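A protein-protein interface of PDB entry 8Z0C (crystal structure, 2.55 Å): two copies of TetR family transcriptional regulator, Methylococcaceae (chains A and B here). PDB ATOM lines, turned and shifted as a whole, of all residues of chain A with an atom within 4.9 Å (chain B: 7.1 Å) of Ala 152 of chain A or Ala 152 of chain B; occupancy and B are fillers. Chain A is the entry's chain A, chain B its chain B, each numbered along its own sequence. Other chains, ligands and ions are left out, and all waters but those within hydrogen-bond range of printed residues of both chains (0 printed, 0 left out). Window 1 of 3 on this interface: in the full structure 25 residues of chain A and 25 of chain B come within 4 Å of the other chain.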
ATOM      1  N   TRP A 148      33.284 -34.952 -10.305  1.00  0.00           N
ATOM      2  CA  TRP A 148      33.917 -34.142 -11.337  1.00  0.00           C
ATOM      3  C   TRP A 148      32.946 -33.853 -12.467  1.00  0.00           C
ATOM      4  O   TRP A 148      33.002 -32.774 -13.072  1.00  0.00           O
ATOM      5  CB  TRP A 148      35.171 -34.819 -11.887  1.00  0.00           C
ATOM      6  CG  TRP A 148      36.435 -34.500 -11.134  1.00  0.00           C
ATOM      7  CD1 TRP A 148      37.392 -35.387 -10.757  1.00  0.00           C
ATOM      8  CD2 TRP A 148      36.881 -33.214 -10.670  1.00  0.00           C
ATOM      9  NE1 TRP A 148      38.402 -34.747 -10.083  1.00  0.00           N
ATOM     10  CE2 TRP A 148      38.112 -33.413 -10.014  1.00  0.00           C
ATOM     11  CE3 TRP A 148      36.362 -31.915 -10.743  1.00  0.00           C
ATOM     12  CZ2 TRP A 148      38.836 -32.363  -9.439  1.00  0.00           C
ATOM     13  CZ3 TRP A 148      37.087 -30.868 -10.168  1.00  0.00           C
ATOM     14  CH2 TRP A 148      38.306 -31.105  -9.529  1.00  0.00           C
ATOM     15  N   ARG A 149      32.029 -34.780 -12.749  1.00  0.00           N
ATOM     16  CA  ARG A 149      31.094 -34.539 -13.835  1.00  0.00           C
ATOM     17  C   ARG A 149      29.925 -33.666 -13.401  1.00  0.00           C
ATOM     18  O   ARG A 149      29.385 -32.918 -14.219  1.00  0.00           O
ATOM     19  CB  ARG A 149      30.596 -35.863 -14.399  1.00  0.00           C
ATOM     20  CG  ARG A 149      31.673 -36.629 -15.145  1.00  0.00           C
ATOM     21  CD  ARG A 149      31.093 -37.770 -15.939  1.00  0.00           C
ATOM     22  NE  ARG A 149      30.391 -38.739 -15.106  1.00  0.00           N
ATOM     23  CZ  ARG A 149      30.869 -39.948 -14.810  1.00  0.00           C
ATOM     24  NH1 ARG A 149      32.064 -40.316 -15.258  1.00  0.00           N
ATOM     25  NH2 ARG A 149      30.151 -40.796 -14.073  1.00  0.00           N
ATOM     26  N   LEU A 150      29.505 -33.741 -12.141  1.00  0.00           N
ATOM     27  CA  LEU A 150      28.488 -32.799 -11.679  1.00  0.00           C
ATOM     28  C   LEU A 150      29.040 -31.363 -11.666  1.00  0.00           C
ATOM     29  O   LEU A 150      28.332 -30.416 -12.022  1.00  0.00           O
ATOM     30  CB  LEU A 150      27.963 -33.212 -10.294  1.00  0.00           C
ATOM     31  CG  LEU A 150      27.411 -34.621 -10.022  1.00  0.00           C
ATOM     32  CD1 LEU A 150      26.871 -34.739  -8.593  1.00  0.00           C
ATOM     33  CD2 LEU A 150      26.343 -35.067 -11.024  1.00  0.00           C
ATOM     34  N   ILE A 151      30.309 -31.185 -11.287  1.00  0.00           N
ATOM     35  CA  ILE A 151      30.920 -29.863 -11.379  1.00  0.00           C
ATOM     36  C   ILE A 151      30.987 -29.416 -12.832  1.00  0.00           C
ATOM     37  O   ILE A 151      30.694 -28.255 -13.161  1.00  0.00           O
ATOM     38  CB  ILE A 151      32.318 -29.872 -10.729  1.00  0.00           C
ATOM     39  CG1 ILE A 151      32.217 -30.084  -9.218  1.00  0.00           C
ATOM     40  CG2 ILE A 151      33.065 -28.578 -11.028  1.00  0.00           C
ATOM     41  CD1 ILE A 151      33.569 -30.295  -8.570  1.00  0.00           C
ATOM     42  N   ALA A 152      31.390 -30.329 -13.722  1.00  0.00           N
ATOM     43  CA  ALA A 152      31.457 -30.007 -15.144  1.00  0.00           C
ATOM     44  C   ALA A 152      30.106 -29.544 -15.649  1.00  0.00           C
ATOM     45  O   ALA A 152      30.007 -28.567 -16.408  1.00  0.00           O
ATOM     46  CB  ALA A 152      31.925 -31.219 -15.951  1.00  0.00           C
ATOM     47  N   PHE A 153      29.049 -30.208 -15.205  1.00  0.00           N
ATOM     48  CA  PHE A 153      27.754 -29.915 -15.782  1.00  0.00           C
ATOM     49  C   PHE A 153      27.200 -28.591 -15.262  1.00  0.00           C
ATOM     50  O   PHE A 153      26.675 -27.789 -16.040  1.00  0.00           O
ATOM     51  CB  PHE A 153      26.776 -31.078 -15.531  1.00  0.00           C
ATOM     52  CG  PHE A 153      25.442 -30.829 -16.123  1.00  0.00           C
ATOM     53  CD1 PHE A 153      25.221 -31.077 -17.465  1.00  0.00           C
ATOM     54  CD2 PHE A 153      24.435 -30.252 -15.366  1.00  0.00           C
ATOM     55  CE1 PHE A 153      24.002 -30.802 -18.039  1.00  0.00           C
ATOM     56  CE2 PHE A 153      23.211 -29.975 -15.930  1.00  0.00           C
ATOM     57  CZ  PHE A 153      22.995 -30.247 -17.273  1.00  0.00           C
ATOM     58  N   VAL A 154      27.307 -28.339 -13.956  1.00  0.00           N
ATOM     59  CA  VAL A 154      26.739 -27.101 -13.423  1.00  0.00           C
ATOM     60  C   VAL A 154      27.550 -25.903 -13.884  1.00  0.00           C
ATOM     61  O   VAL A 154      26.983 -24.835 -14.115  1.00  0.00           O
ATOM     62  CB  VAL A 154      26.606 -27.139 -11.886  1.00  0.00           C
ATOM     63  CG1 VAL A 154      25.575 -28.195 -11.459  1.00  0.00           C
ATOM     64  CG2 VAL A 154      27.955 -27.376 -11.233  1.00  0.00           C
ATOM     65  N   CYS A 155      28.864 -26.060 -14.079  1.00  0.00           N
ATOM     66  CA  CYS A 155      29.642 -24.957 -14.641  1.00  0.00           C
ATOM     67  C   CYS A 155      29.329 -24.770 -16.115  1.00  0.00           C
ATOM     68  O   CYS A 155      29.205 -23.636 -16.588  1.00  0.00           O
ATOM     69  CB  CYS A 155      31.141 -25.188 -14.443  1.00  0.00           C
ATOM     70  SG  CYS A 155      31.757 -24.953 -12.739  1.00  0.00           S
ATOM     71  N   GLY A 156      29.173 -25.871 -16.854  1.00  0.00           N
ATOM     72  CA  GLY A 156      28.872 -25.767 -18.275  1.00  0.00           C
ATOM     73  C   GLY A 156      27.492 -25.200 -18.551  1.00  0.00           C
ATOM     74  O   GLY A 156      27.302 -24.486 -19.537  1.00  0.00           O
ATOM     75  N   LEU A 157      26.506 -25.514 -17.697  1.00  0.00           N
ATOM     76  CA  LEU A 157      25.170 -24.949 -17.889  1.00  0.00           C
ATOM     77  C   LEU A 157      25.175 -23.435 -17.706  1.00  0.00           C
ATOM     78  O   LEU A 157      24.471 -22.709 -18.419  1.00  0.00           O
ATOM     79  CB  LEU A 157      24.167 -25.585 -16.923  1.00  0.00           C
ATOM     80  CG  LEU A 157      22.714 -25.592 -17.419  1.00  0.00           C
ATOM     81  CD1 LEU A 157      22.622 -25.922 -18.918  1.00  0.00           C
ATOM     82  CD2 LEU A 157      21.885 -26.584 -16.598  1.00  0.00           C
ATOM     83  N   ILE A 160      26.650 -21.703 -20.898  1.00  0.00           N
ATOM     84  CA  ILE A 160      25.773 -21.651 -22.064  1.00  0.00           C
ATOM     85  C   ILE A 160      24.670 -20.622 -21.851  1.00  0.00           C
ATOM     86  O   ILE A 160      24.212 -19.978 -22.808  1.00  0.00           O
ATOM     87  CB  ILE A 160      25.186 -23.047 -22.389  1.00  0.00           C
ATOM     88  CG1 ILE A 160      26.238 -24.155 -22.262  1.00  0.00           C
ATOM     89  CG2 ILE A 160      24.629 -23.092 -23.803  1.00  0.00           C
ATOM     90  CD1 ILE A 160      27.368 -24.068 -23.315  1.00  0.00           C
ATOM     91  N   MET B 117      26.797 -22.338 -32.598  1.00  0.00           N
ATOM     92  CA  MET B 117      26.315 -23.134 -31.467  1.00  0.00           C
ATOM     93  C   MET B 117      24.886 -23.618 -31.694  1.00  0.00           C
ATOM     94  O   MET B 117      24.535 -24.744 -31.317  1.00  0.00           O
ATOM     95  CB  MET B 117      26.399 -22.324 -30.166  1.00  0.00           C
ATOM     96  CG  MET B 117      27.819 -22.091 -29.636  1.00  0.00           C
ATOM     97  SD  MET B 117      28.358 -23.357 -28.449  1.00  0.00           S
ATOM     98  CE  MET B 117      26.988 -23.337 -27.313  1.00  0.00           C
ATOM     99  N   TRP B 120      25.176 -26.466 -34.157  1.00  0.00           N
ATOM    100  CA  TRP B 120      25.736 -27.564 -33.375  1.00  0.00           C
ATOM    101  C   TRP B 120      24.639 -28.327 -32.643  1.00  0.00           C
ATOM    102  O   TRP B 120      24.578 -29.562 -32.690  1.00  0.00           O
ATOM    103  CB  TRP B 120      26.749 -27.024 -32.362  1.00  0.00           C
ATOM    104  CG  TRP B 120      27.566 -28.099 -31.668  1.00  0.00           C
ATOM    105  CD1 TRP B 120      27.781 -29.375 -32.109  1.00  0.00           C
ATOM    106  CD2 TRP B 120      28.273 -27.982 -30.420  1.00  0.00           C
ATOM    107  NE1 TRP B 120      28.589 -30.047 -31.229  1.00  0.00           N
ATOM    108  CE2 TRP B 120      28.908 -29.219 -30.184  1.00  0.00           C
ATOM    109  CE3 TRP B 120      28.440 -26.950 -29.485  1.00  0.00           C
ATOM    110  CZ2 TRP B 120      29.688 -29.460 -29.044  1.00  0.00           C
ATOM    111  CZ3 TRP B 120      29.222 -27.187 -28.356  1.00  0.00           C
ATOM    112  CH2 TRP B 120      29.835 -28.437 -28.145  1.00  0.00           C
ATOM    113  N   ILE B 146      18.282 -33.431 -23.976  1.00  0.00           N
ATOM    114  CA  ILE B 146      19.532 -34.175 -23.965  1.00  0.00           C
ATOM    115  C   ILE B 146      20.600 -33.428 -24.753  1.00  0.00           C
ATOM    116  O   ILE B 146      21.774 -33.398 -24.363  1.00  0.00           O
ATOM    117  CB  ILE B 146      19.298 -35.597 -24.510  1.00  0.00           C
ATOM    118  CG1 ILE B 146      18.348 -36.366 -23.581  1.00  0.00           C
ATOM    119  CG2 ILE B 146      20.600 -36.346 -24.654  1.00  0.00           C
ATOM    120  CD1 ILE B 146      17.431 -37.321 -24.288  1.00  0.00           C
ATOM    121  N   ALA B 147      20.209 -32.786 -25.858  1.00  0.00           N
ATOM    122  CA  ALA B 147      21.198 -32.136 -26.720  1.00  0.00           C
ATOM    123  C   ALA B 147      21.837 -30.933 -26.037  1.00  0.00           C
ATOM    124  O   ALA B 147      23.058 -30.767 -26.105  1.00  0.00           O
ATOM    125  CB  ALA B 147      20.572 -31.709 -28.044  1.00  0.00           C
ATOM    126  N   TRP B 148      21.033 -30.084 -25.380  1.00  0.00           N
ATOM    127  CA  TRP B 148      21.597 -28.958 -24.637  1.00  0.00           C
ATOM    128  C   TRP B 148      22.446 -29.439 -23.475  1.00  0.00           C
ATOM    129  O   TRP B 148      23.509 -28.866 -23.204  1.00  0.00           O
ATOM    130  CB  TRP B 148      20.497 -28.039 -24.113  1.00  0.00           C
ATOM    131  CG  TRP B 148      19.912 -27.117 -25.129  1.00  0.00           C
ATOM    132  CD1 TRP B 148      18.602 -27.043 -25.505  1.00  0.00           C
ATOM    133  CD2 TRP B 148      20.604 -26.115 -25.886  1.00  0.00           C
ATOM    134  NE1 TRP B 148      18.433 -26.066 -26.450  1.00  0.00           N
ATOM    135  CE2 TRP B 148      19.645 -25.473 -26.698  1.00  0.00           C
ATOM    136  CE3 TRP B 148      21.940 -25.684 -25.946  1.00  0.00           C
ATOM    137  CZ2 TRP B 148      19.979 -24.430 -27.570  1.00  0.00           C
ATOM    138  CZ3 TRP B 148      22.270 -24.640 -26.818  1.00  0.00           C
ATOM    139  CH2 TRP B 148      21.294 -24.037 -27.619  1.00  0.00           C
ATOM    140  N   ARG B 149      21.994 -30.493 -22.769  1.00  0.00           N
ATOM    141  CA  ARG B 149      22.749 -30.982 -21.620  1.00  0.00           C
ATOM    142  C   ARG B 149      24.040 -31.637 -22.060  1.00  0.00           C
ATOM    143  O   ARG B 149      25.024 -31.643 -21.309  1.00  0.00           O
ATOM    144  CB  ARG B 149      21.922 -31.957 -20.801  1.00  0.00           C
ATOM    145  CG  ARG B 149      20.762 -31.323 -20.061  1.00  0.00           C
ATOM    146  CD  ARG B 149      20.266 -32.232 -18.962  1.00  0.00           C
ATOM    147  NE  ARG B 149      19.631 -33.420 -19.497  1.00  0.00           N
ATOM    148  CZ  ARG B 149      18.324 -33.651 -19.444  1.00  0.00           C
ATOM    149  NH1 ARG B 149      17.518 -32.748 -18.886  1.00  0.00           N
ATOM    150  NH2 ARG B 149      17.828 -34.790 -19.942  1.00  0.00           N
ATOM    151  N   LEU B 150      24.064 -32.175 -23.272  1.00  0.00           N
ATOM    152  CA  LEU B 150      25.316 -32.704 -23.783  1.00  0.00           C
ATOM    153  C   LEU B 150      26.275 -31.573 -24.140  1.00  0.00           C
ATOM    154  O   LEU B 150      27.489 -31.702 -23.940  1.00  0.00           O
ATOM    155  CB  LEU B 150      25.052 -33.604 -24.987  1.00  0.00           C
ATOM    156  CG  LEU B 150      24.506 -35.017 -24.745  1.00  0.00           C
ATOM    157  CD1 LEU B 150      24.522 -35.820 -26.061  1.00  0.00           C
ATOM    158  CD2 LEU B 150      25.276 -35.749 -23.656  1.00  0.00           C
ATOM    159  N   ILE B 151      25.744 -30.457 -24.652  1.00  0.00           N
ATOM    160  CA  ILE B 151      26.579 -29.301 -24.941  1.00  0.00           C
ATOM    161  C   ILE B 151      27.118 -28.703 -23.644  1.00  0.00           C
ATOM    162  O   ILE B 151      28.326 -28.490 -23.498  1.00  0.00           O
ATOM    163  CB  ILE B 151      25.796 -28.266 -25.766  1.00  0.00           C
ATOM    164  CG1 ILE B 151      25.534 -28.793 -27.172  1.00  0.00           C
ATOM    165  CG2 ILE B 151      26.574 -26.911 -25.855  1.00  0.00           C
ATOM    166  CD1 ILE B 151      25.073 -27.714 -28.155  1.00  0.00           C
ATOM    167  N   ALA B 152      26.233 -28.417 -22.684  1.00  0.00           N
ATOM    168  CA  ALA B 152      26.677 -27.891 -21.392  1.00  0.00           C
ATOM    169  C   ALA B 152      27.760 -28.764 -20.774  1.00  0.00           C
ATOM    170  O   ALA B 152      28.681 -28.252 -20.129  1.00  0.00           O
ATOM    171  CB  ALA B 152      25.496 -27.761 -20.406  1.00  0.00           C
ATOM    172  N   PHE B 153      27.692 -30.078 -20.977  1.00  0.00           N
ATOM    173  CA  PHE B 153      28.644 -30.933 -20.290  1.00  0.00           C
ATOM    174  C   PHE B 153      30.028 -30.839 -20.908  1.00  0.00           C
ATOM    175  O   PHE B 153      31.026 -30.827 -20.179  1.00  0.00           O
ATOM    176  CB  PHE B 153      28.188 -32.390 -20.282  1.00  0.00           C
ATOM    177  CG  PHE B 153      29.193 -33.299 -19.631  1.00  0.00           C
ATOM    178  CD1 PHE B 153      29.222 -33.438 -18.250  1.00  0.00           C
ATOM    179  CD2 PHE B 153      30.155 -33.952 -20.396  1.00  0.00           C
ATOM    180  CE1 PHE B 153      30.158 -34.231 -17.642  1.00  0.00           C
ATOM    181  CE2 PHE B 153      31.108 -34.756 -19.797  1.00  0.00           C
ATOM    182  CZ  PHE B 153      31.109 -34.898 -18.414  1.00  0.00           C
ATOM    183  N   VAL B 154      30.122 -30.804 -22.242  1.00  0.00           N
ATOM    184  CA  VAL B 154      31.442 -30.831 -22.875  1.00  0.00           C
ATOM    185  C   VAL B 154      32.134 -29.487 -22.717  1.00  0.00           C
ATOM    186  O   VAL B 154      33.322 -29.427 -22.378  1.00  0.00           O
ATOM    187  CB  VAL B 154      31.371 -31.257 -24.360  1.00  0.00           C
ATOM    188  CG1 VAL B 154      31.259 -32.778 -24.480  1.00  0.00           C
ATOM    189  CG2 VAL B 154      30.239 -30.558 -25.093  1.00  0.00           C
ATOM    190  N   CYS B 155      31.409 -28.388 -22.955  1.00  0.00           N
ATOM    191  CA  CYS B 155      31.946 -27.076 -22.633  1.00  0.00           C
ATOM    192  C   CYS B 155      32.358 -27.018 -21.165  1.00  0.00           C
ATOM    193  O   CYS B 155      33.473 -26.597 -20.835  1.00  0.00           O
ATOM    194  CB  CYS B 155      30.916 -25.995 -22.976  1.00  0.00           C
ATOM    195  SG  CYS B 155      30.463 -25.916 -24.767  1.00  0.00           S
ATOM    196  N   GLY B 156      31.488 -27.494 -20.273  1.00  0.00           N
ATOM    197  CA  GLY B 156      31.804 -27.486 -18.854  1.00  0.00           C
ATOM    198  C   GLY B 156      33.033 -28.295 -18.509  1.00  0.00           C
ATOM    199  O   GLY B 156      33.721 -27.993 -17.536  1.00  0.00           O
ATOM    200  N   LEU B 157      33.335 -29.320 -19.305  1.00  0.00           N
ATOM    201  CA  LEU B 157      34.511 -30.139 -19.045  1.00  0.00           C
ATOM    202  C   LEU B 157      35.786 -29.462 -19.530  1.00  0.00           C
ATOM    203  O   LEU B 157      36.778 -29.407 -18.796  1.00  0.00           O
ATOM    204  CB  LEU B 157      34.356 -31.527 -19.690  1.00  0.00           C
ATOM    205  CG  LEU B 157      35.127 -32.632 -18.962  1.00  0.00           C
ATOM    206  CD1 LEU B 157      35.254 -32.309 -17.454  1.00  0.00           C
ATOM    207  CD2 LEU B 157      34.499 -34.003 -19.189  1.00  0.00           C
ATOM    208  N   GLU B 158      35.797 -28.954 -20.765  1.00  0.00           N
ATOM    209  CA  GLU B 158      36.985 -28.223 -21.196  1.00  0.00           C
ATOM    210  C   GLU B 158      37.265 -27.036 -20.287  1.00  0.00           C
ATOM    211  O   GLU B 158      38.432 -26.731 -20.017  1.00  0.00           O
ATOM    212  CB  GLU B 158      36.886 -27.774 -22.657  1.00  0.00           C
ATOM    213  CG  GLU B 158      37.091 -28.944 -23.625  1.00  0.00           C
ATOM    214  CD  GLU B 158      38.579 -29.262 -23.875  1.00  0.00           C
ATOM    215  OE1 GLU B 158      39.429 -28.557 -23.269  1.00  0.00           O
ATOM    216  OE2 GLU B 158      38.885 -30.243 -24.614  1.00  0.00           O
ATOM    217  N   ILE B 160      36.752 -26.865 -16.967  1.00  0.00           N
ATOM    218  CA  ILE B 160      37.408 -27.307 -15.743  1.00  0.00           C
ATOM    219  C   ILE B 160      38.854 -27.697 -16.029  1.00  0.00           C
ATOM    220  O   ILE B 160      39.757 -27.432 -15.225  1.00  0.00           O
ATOM    221  CB  ILE B 160      36.616 -28.463 -15.106  1.00  0.00           C
ATOM    222  CG1 ILE B 160      35.195 -28.007 -14.810  1.00  0.00           C
ATOM    223  CG2 ILE B 160      37.241 -28.848 -13.811  1.00  0.00           C
ATOM    224  CD1 ILE B 160      35.109 -26.564 -14.259  1.00  0.00           C
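Arg 149 of chain A touches Phe 153 of chain B (CB to CE1, 3.7 Å). Ala 152 of chain A touches Phe 153 of chain B (CB to CE1, 3.9 Å). O of Ala 152 of chain A touches CA of Gly 156 of chain B, at 3.2 Å. Ala 152 of chain A touches Leu 157 of chain B. Gly 156 of chain A touches Ala 152 of chain B. Gly 156 of chain A touches Gly 156 of chain B (CA to CA, 3.4 Å). Ala 152 of chain B touches Leu 157 of chain A (CB to N, 3.7 Å). Ile 160 of chain A touches Ile 151 of chain B (CD1 to CG2, 3.9 Å). Ile 160 of chain A touches Ala 152 of chain B. Ile 160 of chain A touches Cys 155 of chain B (CD1 to SG, 3.9 Å).
Of the 11 printed residues of chain A, 6 touch a printed residue of chain B. Hydrophobic or aromatic side chains of chain B that line the printed part of chain A: Ile 151, Ala 152, Phe 153 and Leu 157. Among the printed residues, no Asp or Glu carboxylate lies within 4 Å of a Lys or Arg side-chain nitrogen of the other chain.
The backbone carbonyl oxygen (O) of Ile 151 of chain B lies within hydrogen-bond range of the side-chain sulfur (SG) of Cys 155 of chain B (3.6 Å).
Ala 152 of chain A touches Phe 153 of chain B, but with the chains exchanged Phe 153 of chain A does not touch Ala 152 of chain B (4.1 Å). Ala 152 of chain A touches Gly 156 of chain B, and with the chains exchanged Gly 156 of chain A touches Ala 152 of chain B. Ala 152 of chain A touches Leu 157 of chain B, and with the chains exchanged Leu 157 of chain A touches Ala 152 of chain B. Ile 160 of chain A touches Ile 151 of chain B, but with the chains exchanged Ile 151 of chain A does not touch Ile 160 of chain B (4.3 Å). Of the 12 pairs that touch across the chains among the printed residues, 8 have their exchanged pair printed and touching as well.
Ala 152 of chain A touches just these residues of chain B: Ala 152, Phe 153, Gly 156 and Leu 157. Ala 152 of chain B touches just these residues of chain A: Ala 152, Gly 156, Leu 157 and Ile 160. Printed residues of chain B within 4 Å of Phe 153 of chain A: Arg 149 (3.5 Å). Printed residues of chain A within 4 Å of Ile 151 of chain B: Ile 160 (3.9 Å). Of the printed residues of chain A, Leu 157 of chain B touches Ala 152 (3.8 Å). Of the printed residues of chain A, Cys 155 of chain B touches Ile 160. Trp 148 of chain A touches none of the printed residues of chain B. Trp 148 of chain B touches none of the printed residues of chain A. The nearest printed residue of chain B that does not touch Arg 149 of chain A is Leu 157 of chain B (5.6 Å).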
